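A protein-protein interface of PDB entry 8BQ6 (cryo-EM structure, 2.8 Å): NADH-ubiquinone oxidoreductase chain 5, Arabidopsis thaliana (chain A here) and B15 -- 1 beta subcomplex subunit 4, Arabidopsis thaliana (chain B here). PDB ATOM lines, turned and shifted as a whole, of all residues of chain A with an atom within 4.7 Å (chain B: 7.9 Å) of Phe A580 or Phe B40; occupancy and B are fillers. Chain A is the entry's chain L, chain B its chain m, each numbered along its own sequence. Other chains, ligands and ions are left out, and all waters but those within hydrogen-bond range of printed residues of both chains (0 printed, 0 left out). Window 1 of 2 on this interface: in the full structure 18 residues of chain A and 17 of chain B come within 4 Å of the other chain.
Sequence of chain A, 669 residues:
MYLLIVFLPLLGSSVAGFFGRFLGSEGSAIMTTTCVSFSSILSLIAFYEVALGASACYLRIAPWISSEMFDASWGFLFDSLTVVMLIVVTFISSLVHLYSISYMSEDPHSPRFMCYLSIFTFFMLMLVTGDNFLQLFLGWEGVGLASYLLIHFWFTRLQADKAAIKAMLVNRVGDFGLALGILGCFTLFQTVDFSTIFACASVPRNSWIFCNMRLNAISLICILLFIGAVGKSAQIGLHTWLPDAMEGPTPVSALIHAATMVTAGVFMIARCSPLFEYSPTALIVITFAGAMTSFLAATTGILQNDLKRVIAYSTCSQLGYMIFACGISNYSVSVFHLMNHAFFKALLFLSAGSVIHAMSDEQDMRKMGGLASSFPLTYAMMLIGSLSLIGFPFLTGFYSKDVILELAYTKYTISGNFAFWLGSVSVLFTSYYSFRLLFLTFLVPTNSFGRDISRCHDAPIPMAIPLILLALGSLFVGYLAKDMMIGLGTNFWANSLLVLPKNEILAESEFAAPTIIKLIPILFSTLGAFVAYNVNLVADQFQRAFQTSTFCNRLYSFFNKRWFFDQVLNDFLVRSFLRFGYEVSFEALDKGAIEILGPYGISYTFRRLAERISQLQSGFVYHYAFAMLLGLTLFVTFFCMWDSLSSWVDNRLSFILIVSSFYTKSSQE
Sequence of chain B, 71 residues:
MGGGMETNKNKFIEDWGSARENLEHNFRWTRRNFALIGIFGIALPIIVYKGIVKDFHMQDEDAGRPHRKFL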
ATOM      1  N   SER A 576     -27.257  22.723  29.442  1.00  0.00           N
ATOM      2  CA  SER A 576     -27.222  22.222  28.071  1.00  0.00           C
ATOM      3  C   SER A 576     -26.496  20.883  27.990  1.00  0.00           C
ATOM      4  O   SER A 576     -26.979  19.938  27.354  1.00  0.00           O
ATOM      5  CB  SER A 576     -26.556  23.245  27.150  1.00  0.00           C
ATOM      6  OG  SER A 576     -27.465  24.253  26.747  1.00  0.00           O
ATOM      7  N   PHE A 577     -25.328  20.782  28.628  1.00  0.00           N
ATOM      8  CA  PHE A 577     -24.556  19.543  28.568  1.00  0.00           C
ATOM      9  C   PHE A 577     -25.213  18.433  29.372  1.00  0.00           C
ATOM     10  O   PHE A 577     -25.186  17.265  28.968  1.00  0.00           O
ATOM     11  CB  PHE A 577     -23.133  19.783  29.063  1.00  0.00           C
ATOM     12  CG  PHE A 577     -22.291  20.541  28.099  1.00  0.00           C
ATOM     13  CD1 PHE A 577     -21.729  21.749  28.452  1.00  0.00           C
ATOM     14  CD2 PHE A 577     -22.068  20.049  26.827  1.00  0.00           C
ATOM     15  CE1 PHE A 577     -20.957  22.451  27.558  1.00  0.00           C
ATOM     16  CE2 PHE A 577     -21.293  20.748  25.929  1.00  0.00           C
ATOM     17  CZ  PHE A 577     -20.738  21.952  26.296  1.00  0.00           C
ATOM     18  N   LEU A 578     -25.788  18.773  30.525  1.00  0.00           N
ATOM     19  CA  LEU A 578     -26.482  17.769  31.324  1.00  0.00           C
ATOM     20  C   LEU A 578     -27.673  17.191  30.571  1.00  0.00           C
ATOM     21  O   LEU A 578     -27.893  15.975  30.583  1.00  0.00           O
ATOM     22  CB  LEU A 578     -26.932  18.385  32.644  1.00  0.00           C
ATOM     23  CG  LEU A 578     -25.901  18.423  33.766  1.00  0.00           C
ATOM     24  CD1 LEU A 578     -26.461  19.243  34.897  1.00  0.00           C
ATOM     25  CD2 LEU A 578     -25.583  17.015  34.240  1.00  0.00           C
ATOM     26  N   ARG A 579     -28.446  18.049  29.901  1.00  0.00           N
ATOM     27  CA  ARG A 579     -29.604  17.585  29.144  1.00  0.00           C
ATOM     28  C   ARG A 579     -29.184  16.775  27.927  1.00  0.00           C
ATOM     29  O   ARG A 579     -29.921  15.889  27.480  1.00  0.00           O
ATOM     30  CB  ARG A 579     -30.450  18.775  28.704  1.00  0.00           C
ATOM     31  CG  ARG A 579     -31.154  19.489  29.829  1.00  0.00           C
ATOM     32  CD  ARG A 579     -32.124  20.509  29.280  1.00  0.00           C
ATOM     33  NE  ARG A 579     -33.125  19.872  28.436  1.00  0.00           N
ATOM     34  CZ  ARG A 579     -33.952  20.521  27.631  1.00  0.00           C
ATOM     35  NH1 ARG A 579     -33.947  21.842  27.555  1.00  0.00           N
ATOM     36  NH2 ARG A 579     -34.810  19.829  26.888  1.00  0.00           N
ATOM     37  N   PHE A 580     -28.026  17.096  27.352  1.00  0.00           N
ATOM     38  CA  PHE A 580     -27.553  16.370  26.180  1.00  0.00           C
ATOM     39  C   PHE A 580     -27.238  14.920  26.519  1.00  0.00           C
ATOM     40  O   PHE A 580     -27.520  14.011  25.729  1.00  0.00           O
ATOM     41  CB  PHE A 580     -26.323  17.060  25.595  1.00  0.00           C
ATOM     42  CG  PHE A 580     -25.771  16.368  24.393  1.00  0.00           C
ATOM     43  CD1 PHE A 580     -24.857  15.338  24.529  1.00  0.00           C
ATOM     44  CD2 PHE A 580     -26.192  16.714  23.128  1.00  0.00           C
ATOM     45  CE1 PHE A 580     -24.362  14.685  23.430  1.00  0.00           C
ATOM     46  CE2 PHE A 580     -25.694  16.063  22.025  1.00  0.00           C
ATOM     47  CZ  PHE A 580     -24.779  15.046  22.178  1.00  0.00           C
ATOM     48  N   GLY A 581     -26.634  14.687  27.684  1.00  0.00           N
ATOM     49  CA  GLY A 581     -26.200  13.345  28.029  1.00  0.00           C
ATOM     50  C   GLY A 581     -27.346  12.392  28.294  1.00  0.00           C
ATOM     51  O   GLY A 581     -27.140  11.180  28.393  1.00  0.00           O
ATOM     52  N   TYR A 582     -28.561  12.916  28.425  1.00  0.00           N
ATOM     53  CA  TYR A 582     -29.717  12.050  28.616  1.00  0.00           C
ATOM     54  C   TYR A 582     -30.606  12.034  27.379  1.00  0.00           C
ATOM     55  O   TYR A 582     -30.892  10.970  26.822  1.00  0.00           O
ATOM     56  CB  TYR A 582     -30.513  12.491  29.847  1.00  0.00           C
ATOM     57  CG  TYR A 582     -31.722  11.628  30.104  1.00  0.00           C
ATOM     58  CD1 TYR A 582     -31.604  10.435  30.801  1.00  0.00           C
ATOM     59  CD2 TYR A 582     -32.978  12.000  29.649  1.00  0.00           C
ATOM     60  CE1 TYR A 582     -32.700   9.638  31.034  1.00  0.00           C
ATOM     61  CE2 TYR A 582     -34.080  11.210  29.879  1.00  0.00           C
ATOM     62  CZ  TYR A 582     -33.935  10.029  30.573  1.00  0.00           C
ATOM     63  OH  TYR A 582     -35.030   9.234  30.807  1.00  0.00           O
ATOM     64  N   GLU A 583     -31.037  13.209  26.929  1.00  0.00           N
ATOM     65  CA  GLU A 583     -32.017  13.270  25.855  1.00  0.00           C
ATOM     66  C   GLU A 583     -31.433  12.946  24.491  1.00  0.00           C
ATOM     67  O   GLU A 583     -32.183  12.552  23.594  1.00  0.00           O
ATOM     68  CB  GLU A 583     -32.662  14.647  25.826  1.00  0.00           C
ATOM     69  CG  GLU A 583     -33.634  14.853  26.958  1.00  0.00           C
ATOM     70  CD  GLU A 583     -33.662  16.276  27.440  1.00  0.00           C
ATOM     71  OE1 GLU A 583     -33.872  17.179  26.606  1.00  0.00           O
ATOM     72  OE2 GLU A 583     -33.494  16.488  28.658  1.00  0.00           O
ATOM     73  N   VAL A 584     -30.126  13.099  24.305  1.00  0.00           N
ATOM     74  CA  VAL A 584     -29.566  12.956  22.969  1.00  0.00           C
ATOM     75  C   VAL A 584     -28.668  11.731  22.901  1.00  0.00           C
ATOM     76  O   VAL A 584     -28.953  10.783  22.162  1.00  0.00           O
ATOM     77  CB  VAL A 584     -28.798  14.223  22.556  1.00  0.00           C
ATOM     78  CG1 VAL A 584     -28.290  14.086  21.135  1.00  0.00           C
ATOM     79  CG2 VAL A 584     -29.686  15.445  22.698  1.00  0.00           C
ATOM     80  N   SER A 585     -27.591  11.732  23.685  1.00  0.00           N
ATOM     81  CA  SER A 585     -26.596  10.674  23.553  1.00  0.00           C
ATOM     82  C   SER A 585     -27.106   9.355  24.117  1.00  0.00           C
ATOM     83  O   SER A 585     -26.673   8.280  23.689  1.00  0.00           O
ATOM     84  CB  SER A 585     -25.293  11.090  24.236  1.00  0.00           C
ATOM     85  OG  SER A 585     -25.466  11.263  25.631  1.00  0.00           O
ATOM     86  N   PHE A 586     -28.045   9.432  25.050  1.00  0.00           N
ATOM     87  CA  PHE A 586     -28.520   8.203  25.724  1.00  0.00           C
ATOM     88  C   PHE A 586     -29.903   7.823  25.208  1.00  0.00           C
ATOM     89  O   PHE A 586     -30.027   6.749  24.656  1.00  0.00           O
ATOM     90  CB  PHE A 586     -28.538   8.437  27.232  1.00  0.00           C
ATOM     91  CG  PHE A 586     -29.112   7.324  28.068  1.00  0.00           C
ATOM     92  CD1 PHE A 586     -28.587   6.043  28.011  1.00  0.00           C
ATOM     93  CD2 PHE A 586     -30.163   7.567  28.936  1.00  0.00           C
ATOM     94  CE1 PHE A 586     -29.111   5.029  28.796  1.00  0.00           C
ATOM     95  CE2 PHE A 586     -30.687   6.552  29.719  1.00  0.00           C
ATOM     96  CZ  PHE A 586     -30.161   5.284  29.647  1.00  0.00           C
ATOM     97  N   LEU A 589     -30.032   8.403  20.956  1.00  0.00           N
ATOM     98  CA  LEU A 589     -29.071   7.590  20.221  1.00  0.00           C
ATOM     99  C   LEU A 589     -28.874   6.209  20.838  1.00  0.00           C
ATOM    100  O   LEU A 589     -29.208   5.202  20.206  1.00  0.00           O
ATOM    101  CB  LEU A 589     -27.734   8.325  20.121  1.00  0.00           C
ATOM    102  CG  LEU A 589     -27.706   9.535  19.181  1.00  0.00           C
ATOM    103  CD1 LEU A 589     -26.418  10.312  19.344  1.00  0.00           C
ATOM    104  CD2 LEU A 589     -27.873   9.095  17.738  1.00  0.00           C
ATOM    105  N   ASN B  33     -37.229  13.674  17.816  1.00  0.00           N
ATOM    106  CA  ASN B  33     -36.215  12.635  17.679  1.00  0.00           C
ATOM    107  C   ASN B  33     -35.548  12.695  16.312  1.00  0.00           C
ATOM    108  O   ASN B  33     -34.328  12.534  16.202  1.00  0.00           O
ATOM    109  CB  ASN B  33     -36.841  11.263  17.911  1.00  0.00           C
ATOM    110  CG  ASN B  33     -36.830  10.862  19.365  1.00  0.00           C
ATOM    111  OD1 ASN B  33     -36.101  11.435  20.174  1.00  0.00           O
ATOM    112  ND2 ASN B  33     -37.641   9.874  19.710  1.00  0.00           N
ATOM    113  N   PHE B  34     -36.336  12.930  15.260  1.00  0.00           N
ATOM    114  CA  PHE B  34     -35.775  13.001  13.915  1.00  0.00           C
ATOM    115  C   PHE B  34     -34.777  14.146  13.800  1.00  0.00           C
ATOM    116  O   PHE B  34     -33.714  13.998  13.188  1.00  0.00           O
ATOM    117  CB  PHE B  34     -36.895  13.148  12.884  1.00  0.00           C
ATOM    118  CG  PHE B  34     -37.272  11.858  12.207  1.00  0.00           C
ATOM    119  CD1 PHE B  34     -36.318  11.095  11.556  1.00  0.00           C
ATOM    120  CD2 PHE B  34     -38.581  11.406  12.229  1.00  0.00           C
ATOM    121  CE1 PHE B  34     -36.665   9.911  10.937  1.00  0.00           C
ATOM    122  CE2 PHE B  34     -38.932  10.225  11.613  1.00  0.00           C
ATOM    123  CZ  PHE B  34     -37.974   9.476  10.965  1.00  0.00           C
ATOM    124  N   ALA B  35     -35.104  15.303  14.383  1.00  0.00           N
ATOM    125  CA  ALA B  35     -34.156  16.411  14.384  1.00  0.00           C
ATOM    126  C   ALA B  35     -32.921  16.079  15.212  1.00  0.00           C
ATOM    127  O   ALA B  35     -31.792  16.347  14.790  1.00  0.00           O
ATOM    128  CB  ALA B  35     -34.825  17.683  14.903  1.00  0.00           C
ATOM    129  N   LEU B  36     -33.115  15.486  16.392  1.00  0.00           N
ATOM    130  CA  LEU B  36     -31.982  15.162  17.253  1.00  0.00           C
ATOM    131  C   LEU B  36     -31.074  14.114  16.621  1.00  0.00           C
ATOM    132  O   LEU B  36     -29.846  14.237  16.678  1.00  0.00           O
ATOM    133  CB  LEU B  36     -32.480  14.684  18.613  1.00  0.00           C
ATOM    134  CG  LEU B  36     -32.375  15.682  19.762  1.00  0.00           C
ATOM    135  CD1 LEU B  36     -32.854  17.052  19.333  1.00  0.00           C
ATOM    136  CD2 LEU B  36     -33.182  15.184  20.937  1.00  0.00           C
ATOM    137  N   ILE B  37     -31.653  13.071  16.028  1.00  0.00           N
ATOM    138  CA  ILE B  37     -30.823  12.038  15.418  1.00  0.00           C
ATOM    139  C   ILE B  37     -30.124  12.580  14.179  1.00  0.00           C
ATOM    140  O   ILE B  37     -28.952  12.279  13.933  1.00  0.00           O
ATOM    141  CB  ILE B  37     -31.659  10.783  15.112  1.00  0.00           C
ATOM    142  CG1 ILE B  37     -32.109  10.127  16.414  1.00  0.00           C
ATOM    143  CG2 ILE B  37     -30.856   9.782  14.309  1.00  0.00           C
ATOM    144  CD1 ILE B  37     -33.195   9.105  16.227  1.00  0.00           C
ATOM    145  N   GLY B  38     -30.817  13.404  13.392  1.00  0.00           N
ATOM    146  CA  GLY B  38     -30.189  13.980  12.215  1.00  0.00           C
ATOM    147  C   GLY B  38     -29.033  14.903  12.555  1.00  0.00           C
ATOM    148  O   GLY B  38     -27.988  14.872  11.900  1.00  0.00           O
ATOM    149  N   ILE B  39     -29.201  15.735  13.581  1.00  0.00           N
ATOM    150  CA  ILE B  39     -28.176  16.717  13.918  1.00  0.00           C
ATOM    151  C   ILE B  39     -26.970  16.048  14.563  1.00  0.00           C
ATOM    152  O   ILE B  39     -25.825  16.265  14.152  1.00  0.00           O
ATOM    153  CB  ILE B  39     -28.764  17.806  14.832  1.00  0.00           C
ATOM    154  CG1 ILE B  39     -29.731  18.695  14.054  1.00  0.00           C
ATOM    155  CG2 ILE B  39     -27.659  18.648  15.426  1.00  0.00           C
ATOM    156  CD1 ILE B  39     -30.756  19.370  14.923  1.00  0.00           C
ATOM    157  N   PHE B  40     -27.203  15.226  15.583  1.00  0.00           N
ATOM    158  CA  PHE B  40     -26.111  14.693  16.385  1.00  0.00           C
ATOM    159  C   PHE B  40     -25.716  13.277  16.004  1.00  0.00           C
ATOM    160  O   PHE B  40     -24.681  12.793  16.474  1.00  0.00           O
ATOM    161  CB  PHE B  40     -26.485  14.737  17.867  1.00  0.00           C
ATOM    162  CG  PHE B  40     -26.639  16.124  18.402  1.00  0.00           C
ATOM    163  CD1 PHE B  40     -25.531  16.916  18.643  1.00  0.00           C
ATOM    164  CD2 PHE B  40     -27.895  16.650  18.632  1.00  0.00           C
ATOM    165  CE1 PHE B  40     -25.677  18.196  19.126  1.00  0.00           C
ATOM    166  CE2 PHE B  40     -28.045  17.929  19.112  1.00  0.00           C
ATOM    167  CZ  PHE B  40     -26.936  18.703  19.362  1.00  0.00           C
ATOM    168  N   GLY B  41     -26.506  12.604  15.178  1.00  0.00           N
ATOM    169  CA  GLY B  41     -26.127  11.289  14.712  1.00  0.00           C
ATOM    170  C   GLY B  41     -25.484  11.319  13.343  1.00  0.00           C
ATOM    171  O   GLY B  41     -24.751  10.396  12.979  1.00  0.00           O
ATOM    172  N   ILE B  42     -25.751  12.373  12.570  1.00  0.00           N
ATOM    173  CA  ILE B  42     -25.293  12.435  11.186  1.00  0.00           C
ATOM    174  C   ILE B  42     -24.530  13.725  10.919  1.00  0.00           C
ATOM    175  O   ILE B  42     -23.379  13.696  10.470  1.00  0.00           O
ATOM    176  CB  ILE B  42     -26.475  12.300  10.210  1.00  0.00           C
ATOM    177  CG1 ILE B  42     -27.058  10.890  10.254  1.00  0.00           C
ATOM    178  CG2 ILE B  42     -26.035  12.608   8.795  1.00  0.00           C
ATOM    179  CD1 ILE B  42     -28.193  10.691   9.271  1.00  0.00           C
ATOM    180  N   ALA B  43     -25.170  14.868  11.177  1.00  0.00           N
ATOM    181  CA  ALA B  43     -24.588  16.146  10.778  1.00  0.00           C
ATOM    182  C   ALA B  43     -23.321  16.456  11.568  1.00  0.00           C
ATOM    183  O   ALA B  43     -22.305  16.863  10.994  1.00  0.00           O
ATOM    184  CB  ALA B  43     -25.614  17.268  10.938  1.00  0.00           C
ATOM    185  N   LEU B  44     -23.366  16.287  12.890  1.00  0.00           N
ATOM    186  CA  LEU B  44     -22.195  16.614  13.704  1.00  0.00           C
ATOM    187  C   LEU B  44     -20.997  15.712  13.421  1.00  0.00           C
ATOM    188  O   LEU B  44     -19.879  16.240  13.290  1.00  0.00           O
ATOM    189  CB  LEU B  44     -22.565  16.607  15.190  1.00  0.00           C
ATOM    190  CG  LEU B  44     -21.368  16.908  16.094  1.00  0.00           C
ATOM    191  CD1 LEU B  44     -21.686  18.010  17.088  1.00  0.00           C
ATOM    192  CD2 LEU B  44     -20.892  15.659  16.806  1.00  0.00           C
ATOM    193  N   PRO B  45     -21.127  14.380  13.342  1.00  0.00           N
ATOM    194  CA  PRO B  45     -19.955  13.579  12.946  1.00  0.00           C
ATOM    195  C   PRO B  45     -19.396  13.946  11.584  1.00  0.00           C
ATOM    196  O   PRO B  45     -18.175  13.896  11.393  1.00  0.00           O
ATOM    197  CB  PRO B  45     -20.488  12.140  12.975  1.00  0.00           C
ATOM    198  CG  PRO B  45     -21.623  12.186  13.911  1.00  0.00           C
ATOM    199  CD  PRO B  45     -22.265  13.516  13.705  1.00  0.00           C
ATOM    200  N   ILE B  46     -20.248  14.311  10.623  1.00  0.00           N
ATOM    201  CA  ILE B  46     -19.733  14.722   9.320  1.00  0.00           C
ATOM    202  C   ILE B  46     -18.964  16.031   9.445  1.00  0.00           C
ATOM    203  O   ILE B  46     -17.952  16.241   8.767  1.00  0.00           O
ATOM    204  CB  ILE B  46     -20.874  14.815   8.289  1.00  0.00           C
ATOM    205  CG1 ILE B  46     -21.378  13.415   7.952  1.00  0.00           C
ATOM    206  CG2 ILE B  46     -20.404  15.491   7.013  1.00  0.00           C
ATOM    207  CD1 ILE B  46     -22.529  13.410   6.989  1.00  0.00           C
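NH2 of Arg A579 is in salt-bridge range of OE1 of Glu A583, 2.8 Å away.
N of Ser A585 sits at hydrogen-bond distance from O of Phe A580.
O of Val A584 sits at hydrogen-bond distance from N of Leu A589, at 2.9 Å.
Among the printed residues, pairs that only touch across the chains: Phe A580 with Phe B40, Val A584 with Phe B40, Glu A583 with Leu B36 and Val A584 with Leu B36.
Of the printed residues of chain B, Phe A580 touches Phe B40.
Of the printed residues of chain B, Glu A583 touches Leu B36 (3.9 Å).
Printed residues of chain B within 4 Å of Val A584: Leu B36 (3.9 Å) and Phe B40 (3.6 Å).
Of the printed residues of chain A, Leu B36 touches Glu A583 and Val A584.
Phe B40 touches two residues of chain A.
The nearest residue of chain A that does not touch Phe B40 is Leu A589 (4.2 Å).
The nearest printed residue of chain B that does not touch Glu A583 is Asn B33 (5.3 Å).
Printed residues of chain A that touch a printed residue of chain B: Phe A580, Glu A583 and Val A584.
Hydrophobic or aromatic side chains of chain A that line the printed part of chain B: Phe A580 and Val A584.
Hydrophobic or aromatic side chains of chain B that line the printed part of chain A: Leu B36 and Phe B40.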
